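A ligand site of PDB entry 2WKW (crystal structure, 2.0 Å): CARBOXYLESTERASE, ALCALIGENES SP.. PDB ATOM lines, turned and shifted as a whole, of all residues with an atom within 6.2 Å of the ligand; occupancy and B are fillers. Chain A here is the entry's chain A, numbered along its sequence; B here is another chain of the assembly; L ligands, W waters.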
ATOM      1  N   GLY A  70      -0.567 -25.640  35.554  1.00  0.00           N
ATOM      2  CA  GLY A  70      -1.066 -26.310  34.332  1.00  0.00           C
ATOM      3  C   GLY A  70      -1.555 -27.730  34.564  1.00  0.00           C
ATOM      4  O   GLY A  70      -2.025 -28.061  35.658  1.00  0.00           O
ATOM      5  N   CYS A  71      -1.434 -28.576  33.541  1.00  0.00           N
ATOM      6  CA  CYS A  71      -1.886 -29.966  33.660  1.00  0.00           C
ATOM      7  C   CYS A  71      -0.958 -30.754  34.541  1.00  0.00           C
ATOM      8  O   CYS A  71       0.183 -30.373  34.745  1.00  0.00           O
ATOM      9  CB  CYS A  71      -1.961 -30.684  32.294  1.00  0.00           C
ATOM     10  SG  CYS A  71      -0.451 -31.587  31.879  1.00  0.00           S
ATOM     11  N   CYS A  72      -1.454 -31.891  35.035  1.00  0.00           N
ATOM     12  CA  CYS A  72      -0.567 -32.965  35.497  1.00  0.00           C
ATOM     13  C   CYS A  72       0.273 -32.561  36.704  1.00  0.00           C
ATOM     14  O   CYS A  72       1.259 -33.221  37.030  1.00  0.00           O
ATOM     15  CB  CYS A  72       0.351 -33.329  34.341  1.00  0.00           C
ATOM     16  SG  CYS A  72      -0.572 -33.432  32.783  1.00  0.00           S
ATOM     17  N   LEU A  73      -0.133 -31.459  37.348  1.00  0.00           N
ATOM     18  CA  LEU A  73       0.621 -30.791  38.428  1.00  0.00           C
ATOM     19  C   LEU A  73      -0.336 -30.095  39.385  1.00  0.00           C
ATOM     20  O   LEU A  73      -1.550 -29.954  39.097  1.00  0.00           O
ATOM     21  CB  LEU A  73       1.582 -29.727  37.841  1.00  0.00           C
ATOM     22  CG  LEU A  73       2.702 -30.172  36.891  1.00  0.00           C
ATOM     23  CD1 LEU A  73       3.141 -29.029  35.921  1.00  0.00           C
ATOM     24  CD2 LEU A  73       3.873 -30.789  37.646  1.00  0.00           C
ATOM     25  N   PHE A 134      -6.324 -38.674  32.778  1.00  0.00           N
ATOM     26  CA  PHE A 134      -5.039 -38.699  32.092  1.00  0.00           C
ATOM     27  C   PHE A 134      -3.917 -38.610  33.133  1.00  0.00           C
ATOM     28  O   PHE A 134      -4.059 -37.908  34.141  1.00  0.00           O
ATOM     29  CB  PHE A 134      -4.960 -37.496  31.141  1.00  0.00           C
ATOM     30  CG  PHE A 134      -3.606 -37.307  30.505  1.00  0.00           C
ATOM     31  CD1 PHE A 134      -2.728 -36.337  30.974  1.00  0.00           C
ATOM     32  CD2 PHE A 134      -3.210 -38.115  29.432  1.00  0.00           C
ATOM     33  CE1 PHE A 134      -1.462 -36.164  30.379  1.00  0.00           C
ATOM     34  CE2 PHE A 134      -1.949 -37.950  28.833  1.00  0.00           C
ATOM     35  CZ  PHE A 134      -1.071 -36.980  29.301  1.00  0.00           C
ATOM     36  N   ALA A 136       0.538 -38.038  32.971  1.00  0.00           N
ATOM     37  CA  ALA A 136       1.687 -37.854  32.080  1.00  0.00           C
ATOM     38  C   ALA A 136       2.795 -38.813  32.472  1.00  0.00           C
ATOM     39  O   ALA A 136       3.258 -38.773  33.618  1.00  0.00           O
ATOM     40  CB  ALA A 136       2.179 -36.408  32.138  1.00  0.00           C
ATOM     41  N   GLY A 137       3.221 -39.667  31.544  1.00  0.00           N
ATOM     42  CA  GLY A 137       4.412 -40.523  31.763  1.00  0.00           C
ATOM     43  C   GLY A 137       5.697 -39.703  31.722  1.00  0.00           C
ATOM     44  O   GLY A 137       5.746 -38.669  31.059  1.00  0.00           O
ATOM     45  N   ALA A 140       7.080 -39.281  27.914  1.00  0.00           N
ATOM     46  CA  ALA A 140       6.297 -38.291  27.169  1.00  0.00           C
ATOM     47  C   ALA A 140       6.472 -36.862  27.729  1.00  0.00           C
ATOM     48  O   ALA A 140       6.587 -35.900  26.954  1.00  0.00           O
ATOM     49  CB  ALA A 140       4.827 -38.679  27.122  1.00  0.00           C
ATOM     50  N   ALA A 141       6.511 -36.703  29.051  1.00  0.00           N
ATOM     51  CA  ALA A 141       6.668 -35.366  29.658  1.00  0.00           C
ATOM     52  C   ALA A 141       8.012 -34.712  29.298  1.00  0.00           C
ATOM     53  O   ALA A 141       8.095 -33.505  29.101  1.00  0.00           O
ATOM     54  CB  ALA A 141       6.514 -35.430  31.152  1.00  0.00           C
ATOM     55  N   ILE A 144       7.586 -33.004  25.965  1.00  0.00           N
ATOM     56  CA  ILE A 144       6.637 -31.871  26.083  1.00  0.00           C
ATOM     57  C   ILE A 144       7.268 -30.712  26.867  1.00  0.00           C
ATOM     58  O   ILE A 144       7.031 -29.534  26.544  1.00  0.00           O
ATOM     59  CB  ILE A 144       5.288 -32.335  26.693  1.00  0.00           C
ATOM     60  CG1 ILE A 144       4.584 -33.297  25.712  1.00  0.00           C
ATOM     61  CG2 ILE A 144       4.413 -31.155  27.018  1.00  0.00           C
ATOM     62  CD1 ILE A 144       3.511 -34.191  26.343  1.00  0.00           C
ATOM     63  N   PHE A 145       8.081 -31.045  27.868  1.00  0.00           N
ATOM     64  CA  PHE A 145       8.755 -30.026  28.684  1.00  0.00           C
ATOM     65  C   PHE A 145       9.957 -29.423  27.938  1.00  0.00           C
ATOM     66  O   PHE A 145      10.508 -28.413  28.366  1.00  0.00           O
ATOM     67  CB  PHE A 145       9.245 -30.592  30.019  1.00  0.00           C
ATOM     68  CG  PHE A 145       8.147 -30.896  31.033  1.00  0.00           C
ATOM     69  CD1 PHE A 145       6.980 -30.129  31.107  1.00  0.00           C
ATOM     70  CD2 PHE A 145       8.315 -31.918  31.971  1.00  0.00           C
ATOM     71  CE1 PHE A 145       6.019 -30.398  32.090  1.00  0.00           C
ATOM     72  CE2 PHE A 145       7.343 -32.189  32.947  1.00  0.00           C
ATOM     73  CZ  PHE A 145       6.201 -31.428  33.010  1.00  0.00           C
ATOM     74  N   MET A 172       4.163 -34.751  39.885  1.00  0.00           N
ATOM     75  CA  MET A 172       3.157 -34.932  38.835  1.00  0.00           C
ATOM     76  C   MET A 172       2.020 -35.864  39.280  1.00  0.00           C
ATOM     77  O   MET A 172       2.247 -36.872  39.937  1.00  0.00           O
ATOM     78  CB  MET A 172       3.813 -35.426  37.546  1.00  0.00           C
ATOM     79  CG  MET A 172       4.940 -34.465  37.080  1.00  0.00           C
ATOM     80  SD  MET A 172       5.482 -34.691  35.390  1.00  0.00           S
ATOM     81  CE  MET A 172       4.005 -34.201  34.490  1.00  0.00           C
ATOM     82  N   HIS A 205      -0.224 -21.024  33.339  1.00  0.00           N
ATOM     83  CA  HIS A 205       0.817 -21.873  32.738  1.00  0.00           C
ATOM     84  C   HIS A 205       0.194 -22.972  31.906  1.00  0.00           C
ATOM     85  O   HIS A 205      -0.618 -23.740  32.410  1.00  0.00           O
ATOM     86  CB  HIS A 205       1.704 -22.501  33.840  1.00  0.00           C
ATOM     87  CG  HIS A 205       2.831 -23.319  33.307  1.00  0.00           C
ATOM     88  ND1 HIS A 205       3.178 -24.556  33.815  1.00  0.00           N
ATOM     89  CD2 HIS A 205       3.718 -23.069  32.314  1.00  0.00           C
ATOM     90  CE1 HIS A 205       4.210 -25.037  33.147  1.00  0.00           C
ATOM     91  NE2 HIS A 205       4.576 -24.145  32.243  1.00  0.00           N
ATOM     92  N   SER A 206       0.589 -23.038  30.625  1.00  0.00           N
ATOM     93  CA  SER A 206       0.377 -24.228  29.782  1.00  0.00           C
ATOM     94  C   SER A 206      -1.133 -24.526  29.632  1.00  0.00           C
ATOM     95  O   SER A 206      -1.861 -23.725  29.042  1.00  0.00           O
ATOM     96  CB  SER A 206       1.160 -25.411  30.357  1.00  0.00           C
ATOM     97  OG  SER A 206       1.421 -26.365  29.333  1.00  0.00           O
ATOM     98  N   GLN A 207      -1.600 -25.635  30.209  1.00  0.00           N
ATOM     99  CA  GLN A 207      -3.039 -25.970  30.217  1.00  0.00           C
ATOM    100  C   GLN A 207      -3.922 -24.787  30.680  1.00  0.00           C
ATOM    101  O   GLN A 207      -4.948 -24.503  30.076  1.00  0.00           O
ATOM    102  CB  GLN A 207      -3.281 -27.190  31.122  1.00  0.00           C
ATOM    103  CG  GLN A 207      -4.751 -27.546  31.354  1.00  0.00           C
ATOM    104  CD  GLN A 207      -4.887 -28.548  32.471  1.00  0.00           C
ATOM    105  OE1 GLN A 207      -4.780 -28.183  33.652  1.00  0.00           O
ATOM    106  NE2 GLN A 207      -5.091 -29.819  32.126  1.00  0.00           N
ATOM    107  N   SER A 208      -3.520 -24.112  31.756  1.00  0.00           N
ATOM    108  CA  SER A 208      -4.278 -22.990  32.282  1.00  0.00           C
ATOM    109  C   SER A 208      -3.904 -21.639  31.627  1.00  0.00           C
ATOM    110  O   SER A 208      -4.419 -20.603  32.017  1.00  0.00           O
ATOM    111  CB  SER A 208      -4.118 -22.903  33.803  1.00  0.00           C
ATOM    112  OG  SER A 208      -2.776 -22.534  34.138  1.00  0.00           O
ATOM    113  N   GLY A 232      -1.087 -23.383  26.321  1.00  0.00           N
ATOM    114  CA  GLY A 232      -1.549 -24.351  25.331  1.00  0.00           C
ATOM    115  C   GLY A 232      -2.258 -23.645  24.172  1.00  0.00           C
ATOM    116  O   GLY A 232      -2.183 -24.085  23.048  1.00  0.00           O
ATOM    117  N   ARG A 261       4.752 -29.526  18.531  1.00  0.00           N
ATOM    118  CA  ARG A 261       3.767 -29.112  19.547  1.00  0.00           C
ATOM    119  C   ARG A 261       3.863 -27.611  19.825  1.00  0.00           C
ATOM    120  O   ARG A 261       2.839 -26.940  19.987  1.00  0.00           O
ATOM    121  CB  ARG A 261       4.006 -29.885  20.851  1.00  0.00           C
ATOM    122  CG  ARG A 261       3.065 -29.509  21.987  1.00  0.00           C
ATOM    123  CD  ARG A 261       3.291 -30.407  23.190  1.00  0.00           C
ATOM    124  NE  ARG A 261       2.109 -30.425  24.038  1.00  0.00           N
ATOM    125  CZ  ARG A 261       1.263 -31.445  24.102  1.00  0.00           C
ATOM    126  NH1 ARG A 261       1.484 -32.552  23.390  1.00  0.00           N
ATOM    127  NH2 ARG A 261       0.210 -31.383  24.890  1.00  0.00           N
ATOM    128  N   TRP A 262       5.090 -27.108  19.888  1.00  0.00           N
ATOM    129  CA  TRP A 262       5.348 -25.781  20.442  1.00  0.00           C
ATOM    130  C   TRP A 262       5.475 -24.653  19.425  1.00  0.00           C
ATOM    131  O   TRP A 262       4.980 -23.541  19.659  1.00  0.00           O
ATOM    132  CB  TRP A 262       6.566 -25.818  21.395  1.00  0.00           C
ATOM    133  CG  TRP A 262       6.188 -26.480  22.684  1.00  0.00           C
ATOM    134  CD1 TRP A 262       6.612 -27.704  23.144  1.00  0.00           C
ATOM    135  CD2 TRP A 262       5.254 -25.985  23.644  1.00  0.00           C
ATOM    136  NE1 TRP A 262       6.001 -27.993  24.360  1.00  0.00           N
ATOM    137  CE2 TRP A 262       5.172 -26.948  24.684  1.00  0.00           C
ATOM    138  CE3 TRP A 262       4.467 -24.818  23.733  1.00  0.00           C
ATOM    139  CZ2 TRP A 262       4.332 -26.780  25.807  1.00  0.00           C
ATOM    140  CZ3 TRP A 262       3.644 -24.650  24.841  1.00  0.00           C
ATOM    141  CH2 TRP A 262       3.583 -25.628  25.865  1.00  0.00           C
ATOM    142  N   ARG A 265       2.338 -22.704  18.530  1.00  0.00           N
ATOM    143  CA  ARG A 265       1.754 -21.961  19.646  1.00  0.00           C
ATOM    144  C   ARG A 265       2.433 -20.610  19.816  1.00  0.00           C
ATOM    145  O   ARG A 265       1.769 -19.593  20.084  1.00  0.00           O
ATOM    146  CB  ARG A 265       1.799 -22.794  20.945  1.00  0.00           C
ATOM    147  CG  ARG A 265       0.833 -24.001  20.938  1.00  0.00           C
ATOM    148  CD  ARG A 265       1.116 -24.911  22.134  1.00  0.00           C
ATOM    149  NE  ARG A 265       0.136 -25.991  22.272  1.00  0.00           N
ATOM    150  CZ  ARG A 265       0.184 -26.928  23.214  1.00  0.00           C
ATOM    151  NH1 ARG A 265       1.163 -26.966  24.118  1.00  0.00           N
ATOM    152  NH2 ARG A 265      -0.773 -27.843  23.258  1.00  0.00           N
ATOM    153  N   HIS A 298       9.944 -25.762  29.456  1.00  0.00           N
ATOM    154  CA  HIS A 298       8.520 -25.456  29.696  1.00  0.00           C
ATOM    155  C   HIS A 298       8.266 -25.176  31.183  1.00  0.00           C
ATOM    156  O   HIS A 298       7.351 -24.427  31.555  1.00  0.00           O
ATOM    157  CB  HIS A 298       7.648 -26.643  29.206  1.00  0.00           C
ATOM    158  CG  HIS A 298       6.181 -26.398  29.301  1.00  0.00           C
ATOM    159  ND1 HIS A 298       5.563 -25.303  28.734  1.00  0.00           N
ATOM    160  CD2 HIS A 298       5.197 -27.107  29.903  1.00  0.00           C
ATOM    161  CE1 HIS A 298       4.274 -25.338  28.990  1.00  0.00           C
ATOM    162  NE2 HIS A 298       4.016 -26.428  29.698  1.00  0.00           N
ATOM    163  N   MET A 299       9.117 -25.768  32.028  1.00  0.00           N
ATOM    164  CA  MET A 299       9.021 -25.609  33.475  1.00  0.00           C
ATOM    165  C   MET A 299       9.979 -24.503  33.919  1.00  0.00           C
ATOM    166  O   MET A 299      10.771 -24.700  34.852  1.00  0.00           O
ATOM    167  CB  MET A 299       9.379 -26.912  34.182  1.00  0.00           C
ATOM    168  CG  MET A 299       8.420 -28.063  33.866  1.00  0.00           C
ATOM    169  SD  MET A 299       6.705 -27.689  34.340  1.00  0.00           S
ATOM    170  CE  MET A 299       6.820 -27.707  36.136  1.00  0.00           C
ATOM    171  N   TYR B  39      -2.054 -38.937  22.774  1.00  0.00           N
ATOM    172  CA  TYR B  39      -1.002 -39.224  23.766  1.00  0.00           C
ATOM    173  C   TYR B  39      -0.697 -40.707  23.831  1.00  0.00           C
ATOM    174  O   TYR B  39      -1.568 -41.533  23.594  1.00  0.00           O
ATOM    175  CB  TYR B  39      -1.405 -38.701  25.156  1.00  0.00           C
ATOM    176  CG  TYR B  39      -1.503 -37.196  25.200  1.00  0.00           C
ATOM    177  CD1 TYR B  39      -2.711 -36.547  24.938  1.00  0.00           C
ATOM    178  CD2 TYR B  39      -0.373 -36.404  25.464  1.00  0.00           C
ATOM    179  CE1 TYR B  39      -2.803 -35.150  24.966  1.00  0.00           C
ATOM    180  CE2 TYR B  39      -0.453 -35.011  25.487  1.00  0.00           C
ATOM    181  CZ  TYR B  39      -1.667 -34.395  25.247  1.00  0.00           C
ATOM    182  OH  TYR B  39      -1.764 -33.027  25.265  1.00  0.00           O
HETATM  183  O1  LIG L   1      -0.232 -28.231  30.916  1.00  0.00           O
HETATM  184  C1  LIG L   1       0.656 -28.842  30.320  1.00  0.00           C
HETATM  185  C2  LIG L   1       0.526 -29.285  28.870  1.00  0.00           C
HETATM  186  C3  LIG L   1      -0.630 -28.591  28.120  1.00  0.00           C
HETATM  187  C4  LIG L   1      -0.395 -28.704  26.622  1.00  0.00           C
HETATM  188  O2  LIG L   1       0.767 -28.784  26.171  1.00  0.00           O
HETATM  189  O3  LIG L   1      -1.394 -28.742  25.874  1.00  0.00           O
HETATM  190  N1  LIG L   1       1.835 -29.134  30.911  1.00  0.00           N
HETATM  191  C5  LIG L   1       2.147 -28.758  32.291  1.00  0.00           C
HETATM  192  C6  LIG L   1       2.898 -29.839  30.210  1.00  0.00           C
HETATM  193  C7  LIG L   1       2.504 -31.255  29.897  1.00  0.00           C
HETATM  194  C8  LIG L   1       1.340 -31.626  29.201  1.00  0.00           C
HETATM  195  N2  LIG L   1       0.406 -30.728  28.736  1.00  0.00           N
HETATM  196  C9  LIG L   1       3.395 -32.238  30.351  1.00  0.00           C
HETATM  197  C10 LIG L   1       3.120 -33.565  30.128  1.00  0.00           C
HETATM  198  C11 LIG L   1       1.963 -33.958  29.442  1.00  0.00           C
HETATM  199  C12 LIG L   1       1.073 -32.981  28.975  1.00  0.00           C
HETATM  200  O   HOH W   1      -3.399 -27.163  26.767  1.00  0.00           O
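The backbone NH (N) of Gln 207 sits at hydrogen-bond distance from an oxygen (O1) of the ligand (3.0 Å). An oxygen (O1) of the ligand is in hydrogen-bond range of the backbone NH (N) of Cys 71. An oxygen (O2) of the ligand is in salt-bridge range of the guanidinium group (NH2) of Arg 261, 3.0 Å away. The guanidinium group (NH1) of Arg 265 is in salt-bridge range of an oxygen (O2) of the ligand (2.8 Å). An oxygen (O1) of the ligand lies close to the side-chain hydroxyl of Ser 206. N2 of the ligand lies close to SG of Cys 71 (3.4 Å).
NE of Arg 265 lies within hydrogen-bond range of O of Gly 232, at 3.1 Å. The backbone NH (N) of His 298 sits at hydrogen-bond distance from the backbone carbonyl oxygen (O) of Phe 145 (2.9 Å). The side-chain hydroxyl of Ser 206 is in hydrogen-bond range of a ring nitrogen (NE2) of His 298, 2.6 Å away. O of Ile 144 is in hydrogen-bond range of NE1 of Trp 262 (2.9 Å). The backbone carbonyl oxygen of Gly 70 lies close to the side-chain amide oxygen of Gln 207, at 3.4 Å. The side-chain amide oxygen (OE1) of Gln 207 lies close to the backbone NH (N) of Cys 71 (3.4 Å). N of Gly 232 lies within hydrogen-bond range of O of Ser 206 (2.8 Å). NH2 of Arg 261 lies within hydrogen-bond range of OH of Tyr 39 of chain B (2.6 Å).
C of Gly 70 touches O1 of the ligand (3.9 Å). Leu 73 touches the ligand (CD1 to C5, 3.8 Å). CB of Ala 136 touches C10 of the ligand, 3.6 Å away. Ile 144 touches the ligand. Phe 145 touches the ligand. His 298 touches the ligand. Hydrophobic or aromatic side chains that line the ligand: Leu 73, Ala 136, Ile 144, Phe 145 and His 298. 11 residues have an atom within 4 Å of the ligand: Gly 70, Cys 71, Leu 73, Ala 136, Ile 144, Phe 145, Ser 206, Gln 207, Arg 261, Arg 265 and His 298. The nearest printed residue that does not touch the ligand is Ala 141 (4.01 Å).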
